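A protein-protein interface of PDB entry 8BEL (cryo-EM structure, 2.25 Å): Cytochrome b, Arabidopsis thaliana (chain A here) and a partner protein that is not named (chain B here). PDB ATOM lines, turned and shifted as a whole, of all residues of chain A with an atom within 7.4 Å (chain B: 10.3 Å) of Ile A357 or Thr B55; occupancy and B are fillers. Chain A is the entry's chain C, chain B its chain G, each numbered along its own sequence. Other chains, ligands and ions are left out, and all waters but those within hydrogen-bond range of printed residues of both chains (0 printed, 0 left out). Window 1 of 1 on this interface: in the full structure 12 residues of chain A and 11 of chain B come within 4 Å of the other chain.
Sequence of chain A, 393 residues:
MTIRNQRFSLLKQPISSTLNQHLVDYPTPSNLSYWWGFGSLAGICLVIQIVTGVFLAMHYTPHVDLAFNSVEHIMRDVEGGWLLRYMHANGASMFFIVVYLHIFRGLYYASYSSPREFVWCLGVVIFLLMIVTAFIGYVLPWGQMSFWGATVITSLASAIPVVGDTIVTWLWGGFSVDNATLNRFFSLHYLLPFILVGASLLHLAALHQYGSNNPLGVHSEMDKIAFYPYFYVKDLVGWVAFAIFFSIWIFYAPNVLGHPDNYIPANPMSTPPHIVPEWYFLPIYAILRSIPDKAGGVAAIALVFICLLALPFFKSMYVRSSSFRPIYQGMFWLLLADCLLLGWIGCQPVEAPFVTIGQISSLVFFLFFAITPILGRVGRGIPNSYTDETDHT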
ATOM      1  N   SER A 290     -20.913  23.415  38.063  1.00  0.00           N
ATOM      2  CA  SER A 290     -20.091  23.207  36.877  1.00  0.00           C
ATOM      3  C   SER A 290     -18.704  23.820  37.017  1.00  0.00           C
ATOM      4  O   SER A 290     -17.795  23.440  36.275  1.00  0.00           O
ATOM      5  CB  SER A 290     -20.788  23.775  35.640  1.00  0.00           C
ATOM      6  OG  SER A 290     -20.937  25.178  35.741  1.00  0.00           O
ATOM      7  N   ALA A 337     -33.707  24.722  25.378  1.00  0.00           N
ATOM      8  CA  ALA A 337     -33.267  23.345  25.581  1.00  0.00           C
ATOM      9  C   ALA A 337     -32.119  23.279  26.582  1.00  0.00           C
ATOM     10  O   ALA A 337     -32.081  22.395  27.445  1.00  0.00           O
ATOM     11  CB  ALA A 337     -32.854  22.718  24.249  1.00  0.00           C
ATOM     12  N   ASP A 338     -31.184  24.220  26.485  1.00  0.00           N
ATOM     13  CA  ASP A 338     -30.040  24.244  27.387  1.00  0.00           C
ATOM     14  C   ASP A 338     -30.469  24.493  28.831  1.00  0.00           C
ATOM     15  O   ASP A 338     -29.922  23.892  29.760  1.00  0.00           O
ATOM     16  CB  ASP A 338     -29.054  25.308  26.918  1.00  0.00           C
ATOM     17  CG  ASP A 338     -27.690  25.149  27.534  1.00  0.00           C
ATOM     18  OD1 ASP A 338     -27.195  24.008  27.604  1.00  0.00           O
ATOM     19  OD2 ASP A 338     -27.117  26.175  27.940  1.00  0.00           O
ATOM     20  N   LEU A 341     -31.962  21.365  30.181  1.00  0.00           N
ATOM     21  CA  LEU A 341     -30.875  20.435  30.467  1.00  0.00           C
ATOM     22  C   LEU A 341     -30.162  20.796  31.766  1.00  0.00           C
ATOM     23  O   LEU A 341     -29.798  19.911  32.544  1.00  0.00           O
ATOM     24  CB  LEU A 341     -29.884  20.417  29.301  1.00  0.00           C
ATOM     25  CG  LEU A 341     -30.202  19.521  28.100  1.00  0.00           C
ATOM     26  CD1 LEU A 341     -28.955  19.287  27.267  1.00  0.00           C
ATOM     27  CD2 LEU A 341     -30.796  18.193  28.545  1.00  0.00           C
ATOM     28  N   LEU A 342     -29.932  22.088  32.005  1.00  0.00           N
ATOM     29  CA  LEU A 342     -29.290  22.502  33.251  1.00  0.00           C
ATOM     30  C   LEU A 342     -30.148  22.132  34.451  1.00  0.00           C
ATOM     31  O   LEU A 342     -29.636  21.658  35.473  1.00  0.00           O
ATOM     32  CB  LEU A 342     -29.010  24.003  33.230  1.00  0.00           C
ATOM     33  CG  LEU A 342     -27.754  24.426  32.462  1.00  0.00           C
ATOM     34  CD1 LEU A 342     -27.792  25.911  32.135  1.00  0.00           C
ATOM     35  CD2 LEU A 342     -26.489  24.063  33.223  1.00  0.00           C
ATOM     36  N   TRP A 344     -32.291  19.613  34.613  1.00  0.00           N
ATOM     37  CA  TRP A 344     -32.199  18.166  34.791  1.00  0.00           C
ATOM     38  C   TRP A 344     -30.858  17.763  35.397  1.00  0.00           C
ATOM     39  O   TRP A 344     -30.798  16.857  36.235  1.00  0.00           O
ATOM     40  CB  TRP A 344     -32.424  17.456  33.454  1.00  0.00           C
ATOM     41  CG  TRP A 344     -32.046  16.002  33.451  1.00  0.00           C
ATOM     42  CD1 TRP A 344     -32.714  14.980  34.055  1.00  0.00           C
ATOM     43  CD2 TRP A 344     -30.914  15.412  32.801  1.00  0.00           C
ATOM     44  NE1 TRP A 344     -32.069  13.791  33.828  1.00  0.00           N
ATOM     45  CE2 TRP A 344     -30.961  14.029  33.059  1.00  0.00           C
ATOM     46  CE3 TRP A 344     -29.867  15.920  32.028  1.00  0.00           C
ATOM     47  CZ2 TRP A 344     -30.001  13.146  32.570  1.00  0.00           C
ATOM     48  CZ3 TRP A 344     -28.914  15.041  31.545  1.00  0.00           C
ATOM     49  CH2 TRP A 344     -28.987  13.670  31.820  1.00  0.00           C
ATOM     50  N   ILE A 345     -29.775  18.427  34.987  1.00  0.00           N
ATOM     51  CA  ILE A 345     -28.444  18.096  35.486  1.00  0.00           C
ATOM     52  C   ILE A 345     -28.330  18.425  36.971  1.00  0.00           C
ATOM     53  O   ILE A 345     -27.712  17.678  37.739  1.00  0.00           O
ATOM     54  CB  ILE A 345     -27.368  18.824  34.656  1.00  0.00           C
ATOM     55  CG1 ILE A 345     -27.195  18.155  33.290  1.00  0.00           C
ATOM     56  CG2 ILE A 345     -26.039  18.858  35.394  1.00  0.00           C
ATOM     57  CD1 ILE A 345     -26.469  16.827  33.343  1.00  0.00           C
ATOM     58  N   GLU A 351     -21.043  13.499  39.281  1.00  0.00           N
ATOM     59  CA  GLU A 351     -20.176  12.430  38.805  1.00  0.00           C
ATOM     60  C   GLU A 351     -20.345  12.320  37.294  1.00  0.00           C
ATOM     61  O   GLU A 351     -21.224  12.951  36.701  1.00  0.00           O
ATOM     62  CB  GLU A 351     -20.491  11.102  39.500  1.00  0.00           C
ATOM     63  CG  GLU A 351     -21.749  10.416  38.998  1.00  0.00           C
ATOM     64  CD  GLU A 351     -22.236   9.330  39.939  1.00  0.00           C
ATOM     65  OE1 GLU A 351     -22.173   9.531  41.170  1.00  0.00           O
ATOM     66  OE2 GLU A 351     -22.679   8.271  39.447  1.00  0.00           O
ATOM     67  N   ALA A 352     -19.491  11.510  36.684  1.00  0.00           N
ATOM     68  CA  ALA A 352     -19.518  11.346  35.239  1.00  0.00           C
ATOM     69  C   ALA A 352     -20.829  10.693  34.806  1.00  0.00           C
ATOM     70  O   ALA A 352     -21.370   9.846  35.526  1.00  0.00           O
ATOM     71  CB  ALA A 352     -18.333  10.502  34.773  1.00  0.00           C
ATOM     72  N   PRO A 353     -21.378  11.068  33.642  1.00  0.00           N
ATOM     73  CA  PRO A 353     -20.868  12.037  32.669  1.00  0.00           C
ATOM     74  C   PRO A 353     -21.373  13.449  32.935  1.00  0.00           C
ATOM     75  O   PRO A 353     -21.201  14.339  32.110  1.00  0.00           O
ATOM     76  CB  PRO A 353     -21.422  11.501  31.343  1.00  0.00           C
ATOM     77  CG  PRO A 353     -22.654  10.668  31.719  1.00  0.00           C
ATOM     78  CD  PRO A 353     -22.694  10.563  33.228  1.00  0.00           C
ATOM     79  N   PHE A 354     -22.006  13.677  34.086  1.00  0.00           N
ATOM     80  CA  PHE A 354     -22.777  14.895  34.289  1.00  0.00           C
ATOM     81  C   PHE A 354     -21.921  16.129  34.541  1.00  0.00           C
ATOM     82  O   PHE A 354     -22.410  17.245  34.338  1.00  0.00           O
ATOM     83  CB  PHE A 354     -23.766  14.694  35.433  1.00  0.00           C
ATOM     84  CG  PHE A 354     -24.697  13.542  35.218  1.00  0.00           C
ATOM     85  CD1 PHE A 354     -25.522  13.502  34.106  1.00  0.00           C
ATOM     86  CD2 PHE A 354     -24.750  12.497  36.122  1.00  0.00           C
ATOM     87  CE1 PHE A 354     -26.382  12.446  33.905  1.00  0.00           C
ATOM     88  CE2 PHE A 354     -25.608  11.438  35.924  1.00  0.00           C
ATOM     89  CZ  PHE A 354     -26.424  11.413  34.812  1.00  0.00           C
ATOM     90  N   VAL A 355     -20.665  15.971  34.956  1.00  0.00           N
ATOM     91  CA  VAL A 355     -19.794  17.132  35.121  1.00  0.00           C
ATOM     92  C   VAL A 355     -19.501  17.774  33.769  1.00  0.00           C
ATOM     93  O   VAL A 355     -19.615  18.995  33.603  1.00  0.00           O
ATOM     94  CB  VAL A 355     -18.500  16.735  35.855  1.00  0.00           C
ATOM     95  CG1 VAL A 355     -17.657  17.963  36.157  1.00  0.00           C
ATOM     96  CG2 VAL A 355     -18.832  15.992  37.135  1.00  0.00           C
ATOM     97  N   THR A 356     -19.131  16.957  32.780  1.00  0.00           N
ATOM     98  CA  THR A 356     -18.869  17.474  31.439  1.00  0.00           C
ATOM     99  C   THR A 356     -20.123  18.078  30.822  1.00  0.00           C
ATOM    100  O   THR A 356     -20.070  19.153  30.210  1.00  0.00           O
ATOM    101  CB  THR A 356     -18.321  16.355  30.549  1.00  0.00           C
ATOM    102  OG1 THR A 356     -17.175  15.768  31.174  1.00  0.00           O
ATOM    103  CG2 THR A 356     -17.928  16.892  29.185  1.00  0.00           C
ATOM    104  N   ILE A 357     -21.260  17.397  30.969  1.00  0.00           N
ATOM    105  CA  ILE A 357     -22.508  17.895  30.401  1.00  0.00           C
ATOM    106  C   ILE A 357     -22.895  19.217  31.049  1.00  0.00           C
ATOM    107  O   ILE A 357     -23.314  20.158  30.366  1.00  0.00           O
ATOM    108  CB  ILE A 357     -23.617  16.835  30.536  1.00  0.00           C
ATOM    109  CG1 ILE A 357     -23.256  15.588  29.722  1.00  0.00           C
ATOM    110  CG2 ILE A 357     -24.951  17.393  30.068  1.00  0.00           C
ATOM    111  CD1 ILE A 357     -24.114  14.386  30.022  1.00  0.00           C
ATOM    112  N   GLY A 358     -22.742  19.316  32.371  1.00  0.00           N
ATOM    113  CA  GLY A 358     -23.033  20.566  33.051  1.00  0.00           C
ATOM    114  C   GLY A 358     -22.118  21.695  32.617  1.00  0.00           C
ATOM    115  O   GLY A 358     -22.565  22.828  32.427  1.00  0.00           O
ATOM    116  N   GLN A 359     -20.828  21.400  32.449  1.00  0.00           N
ATOM    117  CA  GLN A 359     -19.886  22.421  32.004  1.00  0.00           C
ATOM    118  C   GLN A 359     -20.250  22.935  30.615  1.00  0.00           C
ATOM    119  O   GLN A 359     -20.294  24.151  30.377  1.00  0.00           O
ATOM    120  CB  GLN A 359     -18.466  21.854  32.021  1.00  0.00           C
ATOM    121  CG  GLN A 359     -17.666  22.223  33.254  1.00  0.00           C
ATOM    122  CD  GLN A 359     -16.706  21.128  33.686  1.00  0.00           C
ATOM    123  OE1 GLN A 359     -16.423  20.199  32.932  1.00  0.00           O
ATOM    124  NE2 GLN A 359     -16.200  21.237  34.908  1.00  0.00           N
ATOM    125  N   ILE A 360     -20.537  22.018  29.689  1.00  0.00           N
ATOM    126  CA  ILE A 360     -20.894  22.422  28.332  1.00  0.00           C
ATOM    127  C   ILE A 360     -22.206  23.199  28.326  1.00  0.00           C
ATOM    128  O   ILE A 360     -22.351  24.191  27.601  1.00  0.00           O
ATOM    129  CB  ILE A 360     -20.944  21.193  27.406  1.00  0.00           C
ATOM    130  CG1 ILE A 360     -19.534  20.646  27.187  1.00  0.00           C
ATOM    131  CG2 ILE A 360     -21.594  21.536  26.070  1.00  0.00           C
ATOM    132  CD1 ILE A 360     -19.505  19.198  26.784  1.00  0.00           C
ATOM    133  N   SER A 361     -23.180  22.767  29.131  1.00  0.00           N
ATOM    134  CA  SER A 361     -24.455  23.475  29.197  1.00  0.00           C
ATOM    135  C   SER A 361     -24.281  24.888  29.744  1.00  0.00           C
ATOM    136  O   SER A 361     -24.876  25.837  29.225  1.00  0.00           O
ATOM    137  CB  SER A 361     -25.450  22.686  30.045  1.00  0.00           C
ATOM    138  OG  SER A 361     -25.906  21.535  29.361  1.00  0.00           O
ATOM    139  N   SER A 362     -23.469  25.050  30.793  1.00  0.00           N
ATOM    140  CA  SER A 362     -23.199  26.387  31.314  1.00  0.00           C
ATOM    141  C   SER A 362     -22.537  27.261  30.257  1.00  0.00           C
ATOM    142  O   SER A 362     -22.879  28.445  30.101  1.00  0.00           O
ATOM    143  CB  SER A 362     -22.318  26.293  32.561  1.00  0.00           C
ATOM    144  OG  SER A 362     -22.876  25.410  33.513  1.00  0.00           O
ATOM    145  N   LEU A 363     -21.590  26.685  29.511  1.00  0.00           N
ATOM    146  CA  LEU A 363     -20.948  27.429  28.435  1.00  0.00           C
ATOM    147  C   LEU A 363     -21.962  27.879  27.389  1.00  0.00           C
ATOM    148  O   LEU A 363     -21.925  29.027  26.941  1.00  0.00           O
ATOM    149  CB  LEU A 363     -19.851  26.579  27.797  1.00  0.00           C
ATOM    150  CG  LEU A 363     -19.178  27.152  26.550  1.00  0.00           C
ATOM    151  CD1 LEU A 363     -18.632  28.545  26.813  1.00  0.00           C
ATOM    152  CD2 LEU A 363     -18.077  26.225  26.079  1.00  0.00           C
ATOM    153  N   LEU B  47     -34.921  21.938  17.116  1.00  0.00           N
ATOM    154  CA  LEU B  47     -33.872  22.578  17.902  1.00  0.00           C
ATOM    155  C   LEU B  47     -34.150  22.503  19.396  1.00  0.00           C
ATOM    156  O   LEU B  47     -33.212  22.523  20.199  1.00  0.00           O
ATOM    157  CB  LEU B  47     -33.707  24.035  17.472  1.00  0.00           C
ATOM    158  CG  LEU B  47     -33.194  24.282  16.058  1.00  0.00           C
ATOM    159  CD1 LEU B  47     -33.181  25.766  15.752  1.00  0.00           C
ATOM    160  CD2 LEU B  47     -31.799  23.690  15.899  1.00  0.00           C
ATOM    161  N   LEU B  48     -35.420  22.429  19.794  1.00  0.00           N
ATOM    162  CA  LEU B  48     -35.702  22.345  21.223  1.00  0.00           C
ATOM    163  C   LEU B  48     -35.619  20.908  21.730  1.00  0.00           C
ATOM    164  O   LEU B  48     -35.086  20.662  22.816  1.00  0.00           O
ATOM    165  CB  LEU B  48     -37.073  22.943  21.538  1.00  0.00           C
ATOM    166  CG  LEU B  48     -37.648  22.600  22.916  1.00  0.00           C
ATOM    167  CD1 LEU B  48     -36.922  23.378  24.004  1.00  0.00           C
ATOM    168  CD2 LEU B  48     -39.142  22.868  22.979  1.00  0.00           C
ATOM    169  N   VAL B  49     -36.110  19.947  20.955  1.00  0.00           N
ATOM    170  CA  VAL B  49     -36.232  18.576  21.441  1.00  0.00           C
ATOM    171  C   VAL B  49     -34.939  17.790  21.263  1.00  0.00           C
ATOM    172  O   VAL B  49     -34.519  17.079  22.179  1.00  0.00           O
ATOM    173  CB  VAL B  49     -37.420  17.884  20.747  1.00  0.00           C
ATOM    174  CG1 VAL B  49     -37.458  16.409  21.100  1.00  0.00           C
ATOM    175  CG2 VAL B  49     -38.718  18.562  21.144  1.00  0.00           C
ATOM    176  N   THR B  50     -34.286  17.900  20.103  1.00  0.00           N
ATOM    177  CA  THR B  50     -33.133  17.049  19.812  1.00  0.00           C
ATOM    178  C   THR B  50     -32.009  17.163  20.836  1.00  0.00           C
ATOM    179  O   THR B  50     -31.499  16.116  21.267  1.00  0.00           O
ATOM    180  CB  THR B  50     -32.624  17.343  18.398  1.00  0.00           C
ATOM    181  OG1 THR B  50     -33.715  17.272  17.475  1.00  0.00           O
ATOM    182  CG2 THR B  50     -31.558  16.342  17.998  1.00  0.00           C
ATOM    183  N   PRO B  51     -31.560  18.356  21.257  1.00  0.00           N
ATOM    184  CA  PRO B  51     -30.510  18.386  22.289  1.00  0.00           C
ATOM    185  C   PRO B  51     -30.923  17.699  23.579  1.00  0.00           C
ATOM    186  O   PRO B  51     -30.132  16.933  24.141  1.00  0.00           O
ATOM    187  CB  PRO B  51     -30.260  19.888  22.495  1.00  0.00           C
ATOM    188  CG  PRO B  51     -30.749  20.528  21.250  1.00  0.00           C
ATOM    189  CD  PRO B  51     -31.924  19.717  20.824  1.00  0.00           C
ATOM    190  N   VAL B  52     -32.158  17.918  24.037  1.00  0.00           N
ATOM    191  CA  VAL B  52     -32.607  17.337  25.301  1.00  0.00           C
ATOM    192  C   VAL B  52     -32.620  15.815  25.219  1.00  0.00           C
ATOM    193  O   VAL B  52     -32.045  15.124  26.070  1.00  0.00           O
ATOM    194  CB  VAL B  52     -33.994  17.887  25.682  1.00  0.00           C
ATOM    195  CG1 VAL B  52     -34.476  17.242  26.965  1.00  0.00           C
ATOM    196  CG2 VAL B  52     -33.951  19.401  25.827  1.00  0.00           C
ATOM    197  N   VAL B  53     -33.267  15.272  24.187  1.00  0.00           N
ATOM    198  CA  VAL B  53     -33.397  13.823  24.072  1.00  0.00           C
ATOM    199  C   VAL B  53     -32.043  13.184  23.806  1.00  0.00           C
ATOM    200  O   VAL B  53     -31.725  12.125  24.359  1.00  0.00           O
ATOM    201  CB  VAL B  53     -34.427  13.457  22.986  1.00  0.00           C
ATOM    202  CG1 VAL B  53     -34.399  11.964  22.709  1.00  0.00           C
ATOM    203  CG2 VAL B  53     -35.818  13.889  23.416  1.00  0.00           C
ATOM    204  N   GLY B  54     -31.224  13.810  22.959  1.00  0.00           N
ATOM    205  CA  GLY B  54     -29.901  13.274  22.695  1.00  0.00           C
ATOM    206  C   GLY B  54     -29.035  13.225  23.938  1.00  0.00           C
ATOM    207  O   GLY B  54     -28.374  12.220  24.209  1.00  0.00           O
ATOM    208  N   THR B  55     -29.034  14.308  24.719  1.00  0.00           N
ATOM    209  CA  THR B  55     -28.241  14.337  25.942  1.00  0.00           C
ATOM    210  C   THR B  55     -28.750  13.321  26.954  1.00  0.00           C
ATOM    211  O   THR B  55     -27.954  12.623  27.592  1.00  0.00           O
ATOM    212  CB  THR B  55     -28.248  15.747  26.534  1.00  0.00           C
ATOM    213  OG1 THR B  55     -27.884  16.687  25.517  1.00  0.00           O
ATOM    214  CG2 THR B  55     -27.263  15.851  27.681  1.00  0.00           C
ATOM    215  N   TYR B  56     -30.072  13.205  27.096  1.00  0.00           N
ATOM    216  CA  TYR B  56     -30.631  12.216  28.009  1.00  0.00           C
ATOM    217  C   TYR B  56     -30.233  10.803  27.598  1.00  0.00           C
ATOM    218  O   TYR B  56     -29.775  10.007  28.428  1.00  0.00           O
ATOM    219  CB  TYR B  56     -32.152  12.356  28.060  1.00  0.00           C
ATOM    220  CG  TYR B  56     -32.803  11.443  29.066  1.00  0.00           C
ATOM    221  CD1 TYR B  56     -32.900  11.812  30.401  1.00  0.00           C
ATOM    222  CD2 TYR B  56     -33.309  10.208  28.687  1.00  0.00           C
ATOM    223  CE1 TYR B  56     -33.487  10.979  31.328  1.00  0.00           C
ATOM    224  CE2 TYR B  56     -33.896   9.370  29.607  1.00  0.00           C
ATOM    225  CZ  TYR B  56     -33.981   9.759  30.926  1.00  0.00           C
ATOM    226  OH  TYR B  56     -34.568   8.928  31.847  1.00  0.00           O
ATOM    227  N   TRP B  57     -30.385  10.483  26.309  1.00  0.00           N
ATOM    228  CA  TRP B  57     -30.052   9.148  25.827  1.00  0.00           C
ATOM    229  C   TRP B  57     -28.573   8.850  26.015  1.00  0.00           C
ATOM    230  O   TRP B  57     -28.205   7.744  26.425  1.00  0.00           O
ATOM    231  CB  TRP B  57     -30.444   9.003  24.355  1.00  0.00           C
ATOM    232  CG  TRP B  57     -30.642   7.582  23.925  1.00  0.00           C
ATOM    233  CD1 TRP B  57     -31.822   6.896  23.878  1.00  0.00           C
ATOM    234  CD2 TRP B  57     -29.631   6.667  23.480  1.00  0.00           C
ATOM    235  NE1 TRP B  57     -31.609   5.616  23.434  1.00  0.00           N
ATOM    236  CE2 TRP B  57     -30.273   5.450  23.182  1.00  0.00           C
ATOM    237  CE3 TRP B  57     -28.247   6.762  23.303  1.00  0.00           C
ATOM    238  CZ2 TRP B  57     -29.578   4.333  22.719  1.00  0.00           C
ATOM    239  CZ3 TRP B  57     -27.560   5.655  22.848  1.00  0.00           C
ATOM    240  CH2 TRP B  57     -28.225   4.457  22.559  1.00  0.00           C
ATOM    241  N   TYR B  58     -27.709   9.825  25.724  1.00  0.00           N
ATOM    242  CA  TYR B  58     -26.280   9.603  25.902  1.00  0.00           C
ATOM    243  C   TYR B  58     -25.940   9.380  27.370  1.00  0.00           C
ATOM    244  O   TYR B  58     -25.087   8.549  27.692  1.00  0.00           O
ATOM    245  CB  TYR B  58     -25.477  10.775  25.337  1.00  0.00           C
ATOM    246  CG  TYR B  58     -24.042  10.782  25.809  1.00  0.00           C
ATOM    247  CD1 TYR B  58     -23.093   9.962  25.214  1.00  0.00           C
ATOM    248  CD2 TYR B  58     -23.639  11.591  26.862  1.00  0.00           C
ATOM    249  CE1 TYR B  58     -21.784   9.953  25.649  1.00  0.00           C
ATOM    250  CE2 TYR B  58     -22.337  11.587  27.303  1.00  0.00           C
ATOM    251  CZ  TYR B  58     -21.412  10.768  26.695  1.00  0.00           C
ATOM    252  OH  TYR B  58     -20.111  10.768  27.135  1.00  0.00           O
ATOM    253  N   ALA B  59     -26.585  10.124  28.273  1.00  0.00           N
ATOM    254  CA  ALA B  59     -26.323   9.936  29.697  1.00  0.00           C
ATOM    255  C   ALA B  59     -26.741   8.546  30.163  1.00  0.00           C
ATOM    256  O   ALA B  59     -26.004   7.889  30.907  1.00  0.00           O
ATOM    257  CB  ALA B  59     -27.034  11.012  30.515  1.00  0.00           C
ATOM    258  N   GLN B  60     -27.922   8.078  29.741  1.00  0.00           N
ATOM    259  CA  GLN B  60     -28.331   6.722  30.113  1.00  0.00           C
ATOM    260  C   GLN B  60     -27.392   5.675  29.527  1.00  0.00           C
ATOM    261  O   GLN B  60     -27.062   4.685  30.193  1.00  0.00           O
ATOM    262  CB  GLN B  60     -29.773   6.431  29.695  1.00  0.00           C
ATOM    263  CG  GLN B  60     -30.758   7.570  29.806  1.00  0.00           C
ATOM    264  CD  GLN B  60     -30.644   8.324  31.119  1.00  0.00           C
ATOM    265  OE1 GLN B  60     -31.027   7.818  32.170  1.00  0.00           O
ATOM    266  NE2 GLN B  60     -30.129   9.545  31.059  1.00  0.00           N
ATOM    267  N   TYR B  61     -26.960   5.870  28.281  1.00  0.00           N
ATOM    268  CA  TYR B  61     -26.022   4.938  27.665  1.00  0.00           C
ATOM    269  C   TYR B  61     -24.712   4.884  28.443  1.00  0.00           C
ATOM    270  O   TYR B  61     -24.177   3.801  28.717  1.00  0.00           O
ATOM    271  CB  TYR B  61     -25.786   5.353  26.212  1.00  0.00           C
ATOM    272  CG  TYR B  61     -24.699   4.588  25.509  1.00  0.00           C
ATOM    273  CD1 TYR B  61     -24.962   3.362  24.916  1.00  0.00           C
ATOM    274  CD2 TYR B  61     -23.410   5.096  25.426  1.00  0.00           C
ATOM    275  CE1 TYR B  61     -23.968   2.661  24.267  1.00  0.00           C
ATOM    276  CE2 TYR B  61     -22.414   4.401  24.784  1.00  0.00           C
ATOM    277  CZ  TYR B  61     -22.698   3.185  24.204  1.00  0.00           C
ATOM    278  OH  TYR B  61     -21.701   2.489  23.558  1.00  0.00           O
ATOM    279  N   PHE B  62     -24.187   6.054  28.816  1.00  0.00           N
ATOM    280  CA  PHE B  62     -22.960   6.115  29.603  1.00  0.00           C
ATOM    281  C   PHE B  62     -23.134   5.405  30.937  1.00  0.00           C
ATOM    282  O   PHE B  62     -22.262   4.636  31.354  1.00  0.00           O
ATOM    283  CB  PHE B  62     -22.558   7.578  29.808  1.00  0.00           C
ATOM    284  CG  PHE B  62     -21.258   7.772  30.552  1.00  0.00           C
ATOM    285  CD1 PHE B  62     -21.191   7.618  31.930  1.00  0.00           C
ATOM    286  CD2 PHE B  62     -20.115   8.154  29.875  1.00  0.00           C
ATOM    287  CE1 PHE B  62     -20.008   7.813  32.608  1.00  0.00           C
ATOM    288  CE2 PHE B  62     -18.930   8.352  30.550  1.00  0.00           C
ATOM    289  CZ  PHE B  62     -18.877   8.181  31.918  1.00  0.00           C
ATOM    290  N   LYS B  63     -24.257   5.650  31.618  1.00  0.00           N
ATOM    291  CA  LYS B  63     -24.486   5.022  32.915  1.00  0.00           C
ATOM    292  C   LYS B  63     -24.555   3.507  32.792  1.00  0.00           C
ATOM    293  O   LYS B  63     -23.976   2.784  33.610  1.00  0.00           O
ATOM    294  CB  LYS B  63     -25.766   5.570  33.544  1.00  0.00           C
ATOM    295  CG  LYS B  63     -25.651   7.004  34.028  1.00  0.00           C
ATOM    296  CD  LYS B  63     -27.013   7.588  34.363  1.00  0.00           C
ATOM    297  CE  LYS B  63     -27.742   6.739  35.393  1.00  0.00           C
ATOM    298  NZ  LYS B  63     -26.996   6.672  36.679  1.00  0.00           N
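The backbone carbonyl oxygen (O) of Pro B51 is in hydrogen-bond range of the side-chain hydroxyl (OG1) of Thr B55 (2.6 Å). NE2 of Gln B60 is in hydrogen-bond range of O of Tyr B56. O of Ile A357 lies within hydrogen-bond range of OG of Ser A361 (3.1 Å).
Ala A337 touches Val B52 (CB to CG2, 3.8 Å). Val B52 touches Leu A341 (CA to CD2, 3.8 Å). CD1 of Leu A341 touches OG1 of Thr B55, at 3.3 Å. Tyr B56 touches Trp A344 (CD1 to CZ2, 3.9 Å). Ala B59 touches Trp A344 (CB to CH2, 3.5 Å). CZ2 of Trp A344 touches NE2 of Gln B60, at 3.9 Å. Pro A353 touches Phe B62 (CG to CD1, 3.4 Å). Phe A354 touches Ala B59. Phe A354 touches Lys B63 (CZ to CD, 3.9 Å). CG2 of Thr B55 touches CG2 of Ile A357 (3.7 Å).
Ile A357 touches one residue of chain B. Printed residues of chain A within 4 Å of Thr B55: Leu A341 (3.3 Å) and Ile A357 (3.7 Å). Pro A353 touches just one residue of chain B: Phe B62. No residue of chain B comes within 4 Å of Thr A356. No residue of chain B comes within 4 Å of Ile A360. No residue of chain B comes within 4 Å of Ser A361. No residue of chain A comes within 4 Å of Gly B54. Of the printed residues of chain A, Tyr B56 touches Trp A344 (3.9 Å). Printed residues of chain A within 4 Å of Ala B59: Trp A344 (3.5 Å) and Phe A354 (3.7 Å). Printed residues of chain A within 4 Å of Val B52: Ala A337 (3.8 Å) and Leu A341 (3.8 Å). Printed residues of chain A within 4 Å of Gln B60: Trp A344. Pro B51 touches none of the printed residues of chain A. Val B49 touches none of the printed residues of chain A. The nearest residue of chain A that does not touch Thr B55 is Trp A344 (4.3 Å).
Of the 17 printed residues of chain B, 8 touch a printed residue of chain A. Printed residues of chain B that touch a printed residue of chain A: Leu B48, Val B52, Thr B55, Tyr B56, Ala B59, Gln B60, Phe B62 and Lys B63. Hydrophobic or aromatic side chains of chain B that line the printed part of chain A: Leu B48, Val B52, Tyr B56, Ala B59 and Phe B62. Among the printed residues, no Asp or Glu carboxylate lies within 4 Å of a Lys or Arg side-chain nitrogen of the other chain.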
